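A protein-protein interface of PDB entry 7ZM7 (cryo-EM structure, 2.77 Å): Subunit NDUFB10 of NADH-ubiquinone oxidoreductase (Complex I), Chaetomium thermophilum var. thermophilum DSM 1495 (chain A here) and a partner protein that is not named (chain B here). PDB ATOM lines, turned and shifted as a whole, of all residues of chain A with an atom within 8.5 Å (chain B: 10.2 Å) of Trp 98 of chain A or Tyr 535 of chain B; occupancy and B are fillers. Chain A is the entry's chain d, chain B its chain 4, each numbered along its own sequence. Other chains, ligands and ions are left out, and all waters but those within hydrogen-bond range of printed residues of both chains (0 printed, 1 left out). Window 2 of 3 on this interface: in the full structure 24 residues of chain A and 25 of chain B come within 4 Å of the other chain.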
ATOM      1  N   PRO A  18      -8.527  -0.114 -35.051  1.00  0.00           N
ATOM      2  CA  PRO A  18      -7.737  -0.008 -33.818  1.00  0.00           C
ATOM      3  C   PRO A  18      -7.916   1.329 -33.104  1.00  0.00           C
ATOM      4  O   PRO A  18      -7.102   2.253 -33.171  1.00  0.00           O
ATOM      5  CB  PRO A  18      -6.310  -0.213 -34.323  1.00  0.00           C
ATOM      6  CG  PRO A  18      -6.337   0.235 -35.690  1.00  0.00           C
ATOM      7  CD  PRO A  18      -7.667  -0.113 -36.242  1.00  0.00           C
ATOM      8  N   THR A  19      -9.029   1.432 -32.391  1.00  0.00           N
ATOM      9  CA  THR A  19      -9.400   2.657 -31.708  1.00  0.00           C
ATOM     10  C   THR A  19     -10.227   2.309 -30.484  1.00  0.00           C
ATOM     11  O   THR A  19     -10.518   1.147 -30.208  1.00  0.00           O
ATOM     12  CB  THR A  19     -10.188   3.587 -32.626  1.00  0.00           C
ATOM     13  OG1 THR A  19     -10.386   4.846 -31.974  1.00  0.00           O
ATOM     14  CG2 THR A  19     -11.529   2.979 -32.954  1.00  0.00           C
ATOM     15  N   PHE A  20     -10.596   3.337 -29.748  1.00  0.00           N
ATOM     16  CA  PHE A  20     -11.547   3.218 -28.666  1.00  0.00           C
ATOM     17  C   PHE A  20     -12.696   4.192 -28.821  1.00  0.00           C
ATOM     18  O   PHE A  20     -13.635   4.143 -28.022  1.00  0.00           O
ATOM     19  CB  PHE A  20     -10.855   3.436 -27.317  1.00  0.00           C
ATOM     20  CG  PHE A  20      -9.987   2.301 -26.915  1.00  0.00           C
ATOM     21  CD1 PHE A  20     -10.540   1.121 -26.466  1.00  0.00           C
ATOM     22  CD2 PHE A  20      -8.626   2.387 -27.017  1.00  0.00           C
ATOM     23  CE1 PHE A  20      -9.746   0.072 -26.112  1.00  0.00           C
ATOM     24  CE2 PHE A  20      -7.841   1.329 -26.667  1.00  0.00           C
ATOM     25  CZ  PHE A  20      -8.405   0.179 -26.215  1.00  0.00           C
ATOM     26  N   ASP A  21     -12.659   5.058 -29.825  1.00  0.00           N
ATOM     27  CA  ASP A  21     -13.762   5.972 -30.072  1.00  0.00           C
ATOM     28  C   ASP A  21     -15.037   5.189 -30.339  1.00  0.00           C
ATOM     29  O   ASP A  21     -15.061   4.284 -31.178  1.00  0.00           O
ATOM     30  CB  ASP A  21     -13.442   6.876 -31.258  1.00  0.00           C
ATOM     31  CG  ASP A  21     -12.372   7.893 -30.942  1.00  0.00           C
ATOM     32  OD1 ASP A  21     -12.276   8.311 -29.771  1.00  0.00           O
ATOM     33  OD2 ASP A  21     -11.625   8.278 -31.865  1.00  0.00           O
ATOM     34  N   TYR A  25     -17.196   0.315 -23.025  1.00  0.00           N
ATOM     35  CA  TYR A  25     -16.233  -0.464 -22.261  1.00  0.00           C
ATOM     36  C   TYR A  25     -16.897  -1.609 -21.514  1.00  0.00           C
ATOM     37  O   TYR A  25     -16.295  -2.676 -21.369  1.00  0.00           O
ATOM     38  CB  TYR A  25     -15.462   0.435 -21.300  1.00  0.00           C
ATOM     39  CG  TYR A  25     -14.359   1.206 -21.971  1.00  0.00           C
ATOM     40  CD1 TYR A  25     -14.354   1.385 -23.335  1.00  0.00           C
ATOM     41  CD2 TYR A  25     -13.341   1.773 -21.246  1.00  0.00           C
ATOM     42  CE1 TYR A  25     -13.370   2.093 -23.953  1.00  0.00           C
ATOM     43  CE2 TYR A  25     -12.345   2.485 -21.866  1.00  0.00           C
ATOM     44  CZ  TYR A  25     -12.368   2.640 -23.219  1.00  0.00           C
ATOM     45  OH  TYR A  25     -11.390   3.341 -23.859  1.00  0.00           O
ATOM     46  N   ILE A  38      -5.241  -2.630 -31.623  1.00  0.00           N
ATOM     47  CA  ILE A  38      -4.117  -1.709 -31.487  1.00  0.00           C
ATOM     48  C   ILE A  38      -2.802  -2.466 -31.342  1.00  0.00           C
ATOM     49  O   ILE A  38      -1.781  -2.057 -31.900  1.00  0.00           O
ATOM     50  CB  ILE A  38      -4.349  -0.701 -30.339  1.00  0.00           C
ATOM     51  CG1 ILE A  38      -5.546   0.207 -30.615  1.00  0.00           C
ATOM     52  CG2 ILE A  38      -3.154   0.184 -30.101  1.00  0.00           C
ATOM     53  CD1 ILE A  38      -6.834  -0.270 -30.161  1.00  0.00           C
ATOM     54  N   GLN A  42       0.620  -2.056 -34.086  1.00  0.00           N
ATOM     55  CA  GLN A  42       1.959  -1.650 -33.595  1.00  0.00           C
ATOM     56  C   GLN A  42       2.971  -2.739 -33.939  1.00  0.00           C
ATOM     57  O   GLN A  42       4.065  -2.396 -34.381  1.00  0.00           O
ATOM     58  CB  GLN A  42       1.922  -1.456 -32.084  1.00  0.00           C
ATOM     59  CG  GLN A  42       1.038  -0.311 -31.623  1.00  0.00           C
ATOM     60  CD  GLN A  42       0.965  -0.279 -30.118  1.00  0.00           C
ATOM     61  OE1 GLN A  42       1.459  -1.171 -29.437  1.00  0.00           O
ATOM     62  NE2 GLN A  42       0.352   0.764 -29.587  1.00  0.00           N
ATOM     63  N   TYR A  90      -1.728  -0.431 -25.361  1.00  0.00           N
ATOM     64  CA  TYR A  90      -2.997   0.254 -25.541  1.00  0.00           C
ATOM     65  C   TYR A  90      -3.417   1.017 -24.300  1.00  0.00           C
ATOM     66  O   TYR A  90      -4.386   1.773 -24.349  1.00  0.00           O
ATOM     67  CB  TYR A  90      -4.089  -0.756 -25.909  1.00  0.00           C
ATOM     68  CG  TYR A  90      -4.328  -1.826 -24.869  1.00  0.00           C
ATOM     69  CD1 TYR A  90      -5.034  -1.553 -23.709  1.00  0.00           C
ATOM     70  CD2 TYR A  90      -3.863  -3.110 -25.054  1.00  0.00           C
ATOM     71  CE1 TYR A  90      -5.245  -2.518 -22.771  1.00  0.00           C
ATOM     72  CE2 TYR A  90      -4.081  -4.080 -24.118  1.00  0.00           C
ATOM     73  CZ  TYR A  90      -4.776  -3.779 -22.985  1.00  0.00           C
ATOM     74  OH  TYR A  90      -4.997  -4.744 -22.041  1.00  0.00           O
ATOM     75  N   LEU A  91      -2.711   0.831 -23.194  1.00  0.00           N
ATOM     76  CA  LEU A  91      -3.209   1.257 -21.899  1.00  0.00           C
ATOM     77  C   LEU A  91      -3.374   2.757 -21.848  1.00  0.00           C
ATOM     78  O   LEU A  91      -4.320   3.268 -21.243  1.00  0.00           O
ATOM     79  CB  LEU A  91      -2.249   0.790 -20.815  1.00  0.00           C
ATOM     80  CG  LEU A  91      -2.704   0.894 -19.378  1.00  0.00           C
ATOM     81  CD1 LEU A  91      -3.889  -0.012 -19.192  1.00  0.00           C
ATOM     82  CD2 LEU A  91      -1.560   0.497 -18.495  1.00  0.00           C
ATOM     83  N   PHE A  92      -2.452   3.481 -22.468  1.00  0.00           N
ATOM     84  CA  PHE A  92      -2.596   4.918 -22.562  1.00  0.00           C
ATOM     85  C   PHE A  92      -3.800   5.305 -23.412  1.00  0.00           C
ATOM     86  O   PHE A  92      -4.577   6.178 -23.025  1.00  0.00           O
ATOM     87  CB  PHE A  92      -1.318   5.526 -23.123  1.00  0.00           C
ATOM     88  CG  PHE A  92      -1.237   6.979 -22.913  1.00  0.00           C
ATOM     89  CD1 PHE A  92      -1.814   7.835 -23.810  1.00  0.00           C
ATOM     90  CD2 PHE A  92      -0.662   7.491 -21.782  1.00  0.00           C
ATOM     91  CE1 PHE A  92      -1.784   9.153 -23.608  1.00  0.00           C
ATOM     92  CE2 PHE A  92      -0.633   8.824 -21.571  1.00  0.00           C
ATOM     93  CZ  PHE A  92      -1.192   9.658 -22.487  1.00  0.00           C
ATOM     94  N   GLU A  93      -3.968   4.665 -24.567  1.00  0.00           N
ATOM     95  CA  GLU A  93      -5.084   5.028 -25.483  1.00  0.00           C
ATOM     96  C   GLU A  93      -6.430   4.606 -24.881  1.00  0.00           C
ATOM     97  O   GLU A  93      -7.428   5.264 -25.201  1.00  0.00           O
ATOM     98  CB  GLU A  93      -4.890   4.413 -26.868  1.00  0.00           C
ATOM     99  CG  GLU A  93      -4.129   5.294 -27.837  1.00  0.00           C
ATOM    100  CD  GLU A  93      -4.373   4.923 -29.289  1.00  0.00           C
ATOM    101  OE1 GLU A  93      -5.529   5.045 -29.740  1.00  0.00           O
ATOM    102  OE2 GLU A  93      -3.413   4.495 -29.960  1.00  0.00           O
ATOM    103  N   GLN A  94      -6.454   3.544 -24.070  1.00  0.00           N
ATOM    104  CA  GLN A  94      -7.703   3.101 -23.462  1.00  0.00           C
ATOM    105  C   GLN A  94      -8.198   4.091 -22.426  1.00  0.00           C
ATOM    106  O   GLN A  94      -9.404   4.273 -22.267  1.00  0.00           O
ATOM    107  CB  GLN A  94      -7.528   1.725 -22.829  1.00  0.00           C
ATOM    108  CG  GLN A  94      -8.828   1.060 -22.470  1.00  0.00           C
ATOM    109  CD  GLN A  94      -8.648  -0.335 -21.970  1.00  0.00           C
ATOM    110  OE1 GLN A  94      -8.524  -1.266 -22.748  1.00  0.00           O
ATOM    111  NE2 GLN A  94      -8.646  -0.500 -20.664  1.00  0.00           N
ATOM    112  N   GLN A  95      -7.282   4.736 -21.716  1.00  0.00           N
ATOM    113  CA  GLN A  95      -7.604   5.558 -20.565  1.00  0.00           C
ATOM    114  C   GLN A  95      -7.620   7.039 -20.860  1.00  0.00           C
ATOM    115  O   GLN A  95      -7.857   7.823 -19.943  1.00  0.00           O
ATOM    116  CB  GLN A  95      -6.606   5.314 -19.453  1.00  0.00           C
ATOM    117  CG  GLN A  95      -6.566   3.933 -18.916  1.00  0.00           C
ATOM    118  CD  GLN A  95      -5.464   3.789 -17.927  1.00  0.00           C
ATOM    119  OE1 GLN A  95      -4.769   4.753 -17.630  1.00  0.00           O
ATOM    120  NE2 GLN A  95      -5.279   2.591 -17.415  1.00  0.00           N
ATOM    121  N   ASN A  96      -7.342   7.445 -22.090  1.00  0.00           N
ATOM    122  CA  ASN A  96      -7.349   8.846 -22.481  1.00  0.00           C
ATOM    123  C   ASN A  96      -8.101   8.961 -23.791  1.00  0.00           C
ATOM    124  O   ASN A  96      -7.943   8.109 -24.667  1.00  0.00           O
ATOM    125  CB  ASN A  96      -5.932   9.389 -22.652  1.00  0.00           C
ATOM    126  CG  ASN A  96      -5.116   9.310 -21.390  1.00  0.00           C
ATOM    127  OD1 ASN A  96      -5.103  10.237 -20.589  1.00  0.00           O
ATOM    128  ND2 ASN A  96      -4.413   8.208 -21.212  1.00  0.00           N
ATOM    129  N   TYR A  97      -8.924   9.988 -23.932  1.00  0.00           N
ATOM    130  CA  TYR A  97      -9.475  10.350 -25.233  1.00  0.00           C
ATOM    131  C   TYR A  97      -8.824  11.628 -25.731  1.00  0.00           C
ATOM    132  O   TYR A  97      -8.701  12.604 -24.992  1.00  0.00           O
ATOM    133  CB  TYR A  97     -11.004  10.466 -25.199  1.00  0.00           C
ATOM    134  CG  TYR A  97     -11.559  11.525 -24.300  1.00  0.00           C
ATOM    135  CD1 TYR A  97     -11.754  12.822 -24.743  1.00  0.00           C
ATOM    136  CD2 TYR A  97     -11.862  11.232 -22.984  1.00  0.00           C
ATOM    137  CE1 TYR A  97     -12.252  13.795 -23.899  1.00  0.00           C
ATOM    138  CE2 TYR A  97     -12.368  12.192 -22.136  1.00  0.00           C
ATOM    139  CZ  TYR A  97     -12.555  13.471 -22.593  1.00  0.00           C
ATOM    140  OH  TYR A  97     -13.057  14.426 -21.743  1.00  0.00           O
ATOM    141  N   TRP A  98      -8.347  11.580 -26.965  1.00  0.00           N
ATOM    142  CA  TRP A  98      -7.697  12.693 -27.634  1.00  0.00           C
ATOM    143  C   TRP A  98      -8.361  12.908 -28.979  1.00  0.00           C
ATOM    144  O   TRP A  98      -8.755  11.946 -29.643  1.00  0.00           O
ATOM    145  CB  TRP A  98      -6.210  12.432 -27.840  1.00  0.00           C
ATOM    146  CG  TRP A  98      -5.548  13.466 -28.686  1.00  0.00           C
ATOM    147  CD1 TRP A  98      -4.960  14.614 -28.265  1.00  0.00           C
ATOM    148  CD2 TRP A  98      -5.413  13.445 -30.100  1.00  0.00           C
ATOM    149  NE1 TRP A  98      -4.469  15.312 -29.331  1.00  0.00           N
ATOM    150  CE2 TRP A  98      -4.738  14.613 -30.472  1.00  0.00           C
ATOM    151  CE3 TRP A  98      -5.807  12.552 -31.095  1.00  0.00           C
ATOM    152  CZ2 TRP A  98      -4.444  14.908 -31.786  1.00  0.00           C
ATOM    153  CZ3 TRP A  98      -5.509  12.841 -32.390  1.00  0.00           C
ATOM    154  CH2 TRP A  98      -4.835  14.008 -32.731  1.00  0.00           C
ATOM    155  N   SER A  99      -8.474  14.166 -29.386  1.00  0.00           N
ATOM    156  CA  SER A  99      -9.127  14.511 -30.636  1.00  0.00           C
ATOM    157  C   SER A  99      -8.252  15.470 -31.425  1.00  0.00           C
ATOM    158  O   SER A  99      -7.364  16.127 -30.877  1.00  0.00           O
ATOM    159  CB  SER A  99     -10.507  15.132 -30.394  1.00  0.00           C
ATOM    160  OG  SER A  99     -11.138  15.451 -31.620  1.00  0.00           O
ATOM    161  N   LYS A 100      -8.523  15.549 -32.729  1.00  0.00           N
ATOM    162  CA  LYS A 100      -7.762  16.448 -33.591  1.00  0.00           C
ATOM    163  C   LYS A 100      -7.905  17.899 -33.147  1.00  0.00           C
ATOM    164  O   LYS A 100      -6.930  18.658 -33.160  1.00  0.00           O
ATOM    165  CB  LYS A 100      -8.215  16.291 -35.042  1.00  0.00           C
ATOM    166  N   GLU A 101      -9.108  18.301 -32.750  1.00  0.00           N
ATOM    167  CA  GLU A 101      -9.351  19.669 -32.310  1.00  0.00           C
ATOM    168  C   GLU A 101      -8.587  19.988 -31.030  1.00  0.00           C
ATOM    169  O   GLU A 101      -7.702  20.844 -31.020  1.00  0.00           O
ATOM    170  CB  GLU A 101     -10.848  19.903 -32.099  1.00  0.00           C
ATOM    171  N   TYR B 527       2.942   1.349 -20.968  1.00  0.00           N
ATOM    172  CA  TYR B 527       2.205   2.602 -20.895  1.00  0.00           C
ATOM    173  C   TYR B 527       2.892   3.630 -21.780  1.00  0.00           C
ATOM    174  O   TYR B 527       4.013   4.044 -21.486  1.00  0.00           O
ATOM    175  CB  TYR B 527       2.149   3.088 -19.452  1.00  0.00           C
ATOM    176  CG  TYR B 527       1.230   4.240 -19.167  1.00  0.00           C
ATOM    177  CD1 TYR B 527      -0.126   4.129 -19.363  1.00  0.00           C
ATOM    178  CD2 TYR B 527       1.723   5.430 -18.656  1.00  0.00           C
ATOM    179  CE1 TYR B 527      -0.963   5.171 -19.080  1.00  0.00           C
ATOM    180  CE2 TYR B 527       0.897   6.470 -18.369  1.00  0.00           C
ATOM    181  CZ  TYR B 527      -0.450   6.342 -18.587  1.00  0.00           C
ATOM    182  OH  TYR B 527      -1.296   7.385 -18.304  1.00  0.00           O
ATOM    183  N   GLY B 528       2.235   4.042 -22.851  1.00  0.00           N
ATOM    184  CA  GLY B 528       2.750   5.139 -23.641  1.00  0.00           C
ATOM    185  C   GLY B 528       2.128   5.216 -25.014  1.00  0.00           C
ATOM    186  O   GLY B 528       1.417   4.328 -25.458  1.00  0.00           O
ATOM    187  N   ILE B 529       2.429   6.319 -25.689  1.00  0.00           N
ATOM    188  CA  ILE B 529       2.016   6.553 -27.066  1.00  0.00           C
ATOM    189  C   ILE B 529       3.149   7.242 -27.798  1.00  0.00           C
ATOM    190  O   ILE B 529       3.982   7.914 -27.191  1.00  0.00           O
ATOM    191  CB  ILE B 529       0.718   7.397 -27.167  1.00  0.00           C
ATOM    192  CG1 ILE B 529       0.911   8.773 -26.547  1.00  0.00           C
ATOM    193  CG2 ILE B 529      -0.467   6.688 -26.606  1.00  0.00           C
ATOM    194  CD1 ILE B 529      -0.216   9.682 -26.823  1.00  0.00           C
ATOM    195  N   GLU B 530       3.174   7.060 -29.110  1.00  0.00           N
ATOM    196  CA  GLU B 530       4.035   7.749 -30.053  1.00  0.00           C
ATOM    197  C   GLU B 530       3.188   8.624 -30.964  1.00  0.00           C
ATOM    198  O   GLU B 530       2.039   8.285 -31.262  1.00  0.00           O
ATOM    199  CB  GLU B 530       4.843   6.739 -30.880  1.00  0.00           C
ATOM    200  CG  GLU B 530       5.732   5.800 -30.084  1.00  0.00           C
ATOM    201  CD  GLU B 530       6.550   6.509 -29.015  1.00  0.00           C
ATOM    202  OE1 GLU B 530       7.548   7.159 -29.383  1.00  0.00           O
ATOM    203  OE2 GLU B 530       6.225   6.412 -27.818  1.00  0.00           O
ATOM    204  N   PRO B 531       3.715   9.758 -31.434  1.00  0.00           N
ATOM    205  CA  PRO B 531       2.825  10.796 -31.974  1.00  0.00           C
ATOM    206  C   PRO B 531       2.140  10.425 -33.271  1.00  0.00           C
ATOM    207  O   PRO B 531       0.993  10.828 -33.479  1.00  0.00           O
ATOM    208  CB  PRO B 531       3.747  11.999 -32.164  1.00  0.00           C
ATOM    209  CG  PRO B 531       5.125  11.497 -31.988  1.00  0.00           C
ATOM    210  CD  PRO B 531       5.126  10.048 -31.704  1.00  0.00           C
ATOM    211  N   ASN B 532       2.793   9.656 -34.135  1.00  0.00           N
ATOM    212  CA  ASN B 532       2.175   9.382 -35.456  1.00  0.00           C
ATOM    213  C   ASN B 532       1.531   7.996 -35.454  1.00  0.00           C
ATOM    214  O   ASN B 532       0.859   7.659 -36.439  1.00  0.00           O
ATOM    215  CB  ASN B 532       3.177   9.635 -36.580  1.00  0.00           C
ATOM    216  CG  ASN B 532       3.571  11.093 -36.688  1.00  0.00           C
ATOM    217  OD1 ASN B 532       4.442  11.563 -35.961  1.00  0.00           O
ATOM    218  ND2 ASN B 532       2.927  11.817 -37.586  1.00  0.00           N
ATOM    219  N   ALA B 533       1.719   7.237 -34.376  1.00  0.00           N
ATOM    220  CA  ALA B 533       1.157   5.873 -34.283  1.00  0.00           C
ATOM    221  C   ALA B 533      -0.083   5.828 -33.395  1.00  0.00           C
ATOM    222  O   ALA B 533      -0.710   4.765 -33.339  1.00  0.00           O
ATOM    223  CB  ALA B 533       2.215   4.969 -33.706  1.00  0.00           C
ATOM    224  N   SER B 534      -0.412   6.911 -32.695  1.00  0.00           N
ATOM    225  CA  SER B 534      -1.538   6.794 -31.742  1.00  0.00           C
ATOM    226  C   SER B 534      -2.820   7.447 -32.239  1.00  0.00           C
ATOM    227  O   SER B 534      -2.744   8.224 -33.205  1.00  0.00           O
ATOM    228  CB  SER B 534      -1.151   7.351 -30.403  1.00  0.00           C
ATOM    229  OG  SER B 534      -0.460   8.583 -30.536  1.00  0.00           O
ATOM    230  N   TYR B 535      -3.953   7.092 -31.639  1.00  0.00           N
ATOM    231  CA  TYR B 535      -5.224   7.760 -31.923  1.00  0.00           C
ATOM    232  C   TYR B 535      -5.531   7.760 -33.419  1.00  0.00           C
ATOM    233  O   TYR B 535      -5.684   8.800 -34.058  1.00  0.00           O
ATOM    234  CB  TYR B 535      -5.230   9.172 -31.347  1.00  0.00           C
ATOM    235  CG  TYR B 535      -5.265   9.176 -29.850  1.00  0.00           C
ATOM    236  CD1 TYR B 535      -6.390   8.768 -29.177  1.00  0.00           C
ATOM    237  CD2 TYR B 535      -4.165   9.560 -29.111  1.00  0.00           C
ATOM    238  CE1 TYR B 535      -6.424   8.747 -27.820  1.00  0.00           C
ATOM    239  CE2 TYR B 535      -4.193   9.532 -27.756  1.00  0.00           C
ATOM    240  CZ  TYR B 535      -5.329   9.127 -27.115  1.00  0.00           C
ATOM    241  OH  TYR B 535      -5.392   9.108 -25.751  1.00  0.00           O
ATOM    242  N   LEU B 536      -5.629   6.556 -33.968  1.00  0.00           N
ATOM    243  CA  LEU B 536      -5.764   6.397 -35.405  1.00  0.00           C
ATOM    244  C   LEU B 536      -7.200   6.648 -35.847  1.00  0.00           C
ATOM    245  O   LEU B 536      -8.147   6.524 -35.068  1.00  0.00           O
ATOM    246  CB  LEU B 536      -5.328   4.997 -35.817  1.00  0.00           C
ATOM    247  CG  LEU B 536      -3.932   4.591 -35.358  1.00  0.00           C
ATOM    248  CD1 LEU B 536      -3.488   3.339 -36.094  1.00  0.00           C
ATOM    249  CD2 LEU B 536      -2.937   5.719 -35.560  1.00  0.00           C
ATOM    250  N   THR B 537      -7.358   7.002 -37.117  1.00  0.00           N
ATOM    251  CA  THR B 537      -8.682   7.237 -37.680  1.00  0.00           C
ATOM    252  C   THR B 537      -8.922   6.358 -38.901  1.00  0.00           C
ATOM    253  O   THR B 537     -10.044   5.918 -39.150  1.00  0.00           O
ATOM    254  CB  THR B 537      -8.872   8.706 -38.075  1.00  0.00           C
ATOM    255  OG1 THR B 537      -7.837   9.094 -38.985  1.00  0.00           O
ATOM    256  CG2 THR B 537      -8.815   9.595 -36.845  1.00  0.00           C
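N of Tyr 535 of chain B sits at hydrogen-bond distance from OE2 of Glu 93 of chain A (3.1 Å).
O of Asn 96 of chain A is in hydrogen-bond range of OH of Tyr 535 of chain B (2.9 Å).
The side-chain amide nitrogen (ND2) of Asn 96 of chain A is in hydrogen-bond range of the backbone carbonyl oxygen (O) of Phe 92 of chain A (2.7 Å).
O of Glu 530 of chain B lies within hydrogen-bond range of OG of Ser 534 of chain B (2.6 Å).
Tyr 527 of chain B touches Phe 92 of chain A (CZ to CD2, 3.4 Å).
Phe 92 of chain A touches Gly 528 of chain B (CB to O, 3.8 Å).
CG2 of Ile 529 of chain B touches CD1 of Phe 92 of chain A (3.3 Å).
Glu 93 of chain A touches Ser 534 of chain B (OE2 to CA, 3.5 Å).
Trp 98 of chain A touches Tyr 535 of chain B (CE3 to CB, 3.4 Å).
Leu 91 of chain A touches none of the printed residues of chain B.
Printed residues of chain B within 4 Å of Phe 92 of chain A: Tyr 527, Gly 528 and Ile 529.
Of chain B, only Ser 534 (3.5 Å) and Tyr 535 (3.1 Å) come within 4 Å of Glu 93 of chain A.
Of chain B, only Tyr 535 (2.9 Å) comes within 4 Å of Asn 96 of chain A.
Trp 98 of chain A touches just one residue of chain B: Tyr 535 (3.4 Å).
No residue of chain B comes within 4 Å of Ser 99 of chain A.
No residue of chain B comes within 4 Å of Lys 100 of chain A.
Glu 101 of chain A touches none of the printed residues of chain B.
Of the printed residues of chain A, Tyr 527 of chain B touches Phe 92 (3.4 Å).
Of the printed residues of chain A, Gly 528 of chain B touches Phe 92.
Of the printed residues of chain A, Ile 529 of chain B touches Phe 92.
Of chain A, only Glu 93 (3.1 Å), Asn 96 (2.9 Å) and Trp 98 (3.4 Å) come within 4 Å of Tyr 535 of chain B.
Of the 11 printed residues of chain B, 5 touch a printed residue of chain A.
Printed residues of chain B that touch a printed residue of chain A: Tyr 527, Gly 528, Ile 529, Ser 534 and Tyr 535.
Among the printed residues, 7 pairs touch across the chains.
Among the printed residues, no Asp or Glu carboxylate lies within 4 Å of a Lys or Arg side-chain nitrogen of the other chain.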
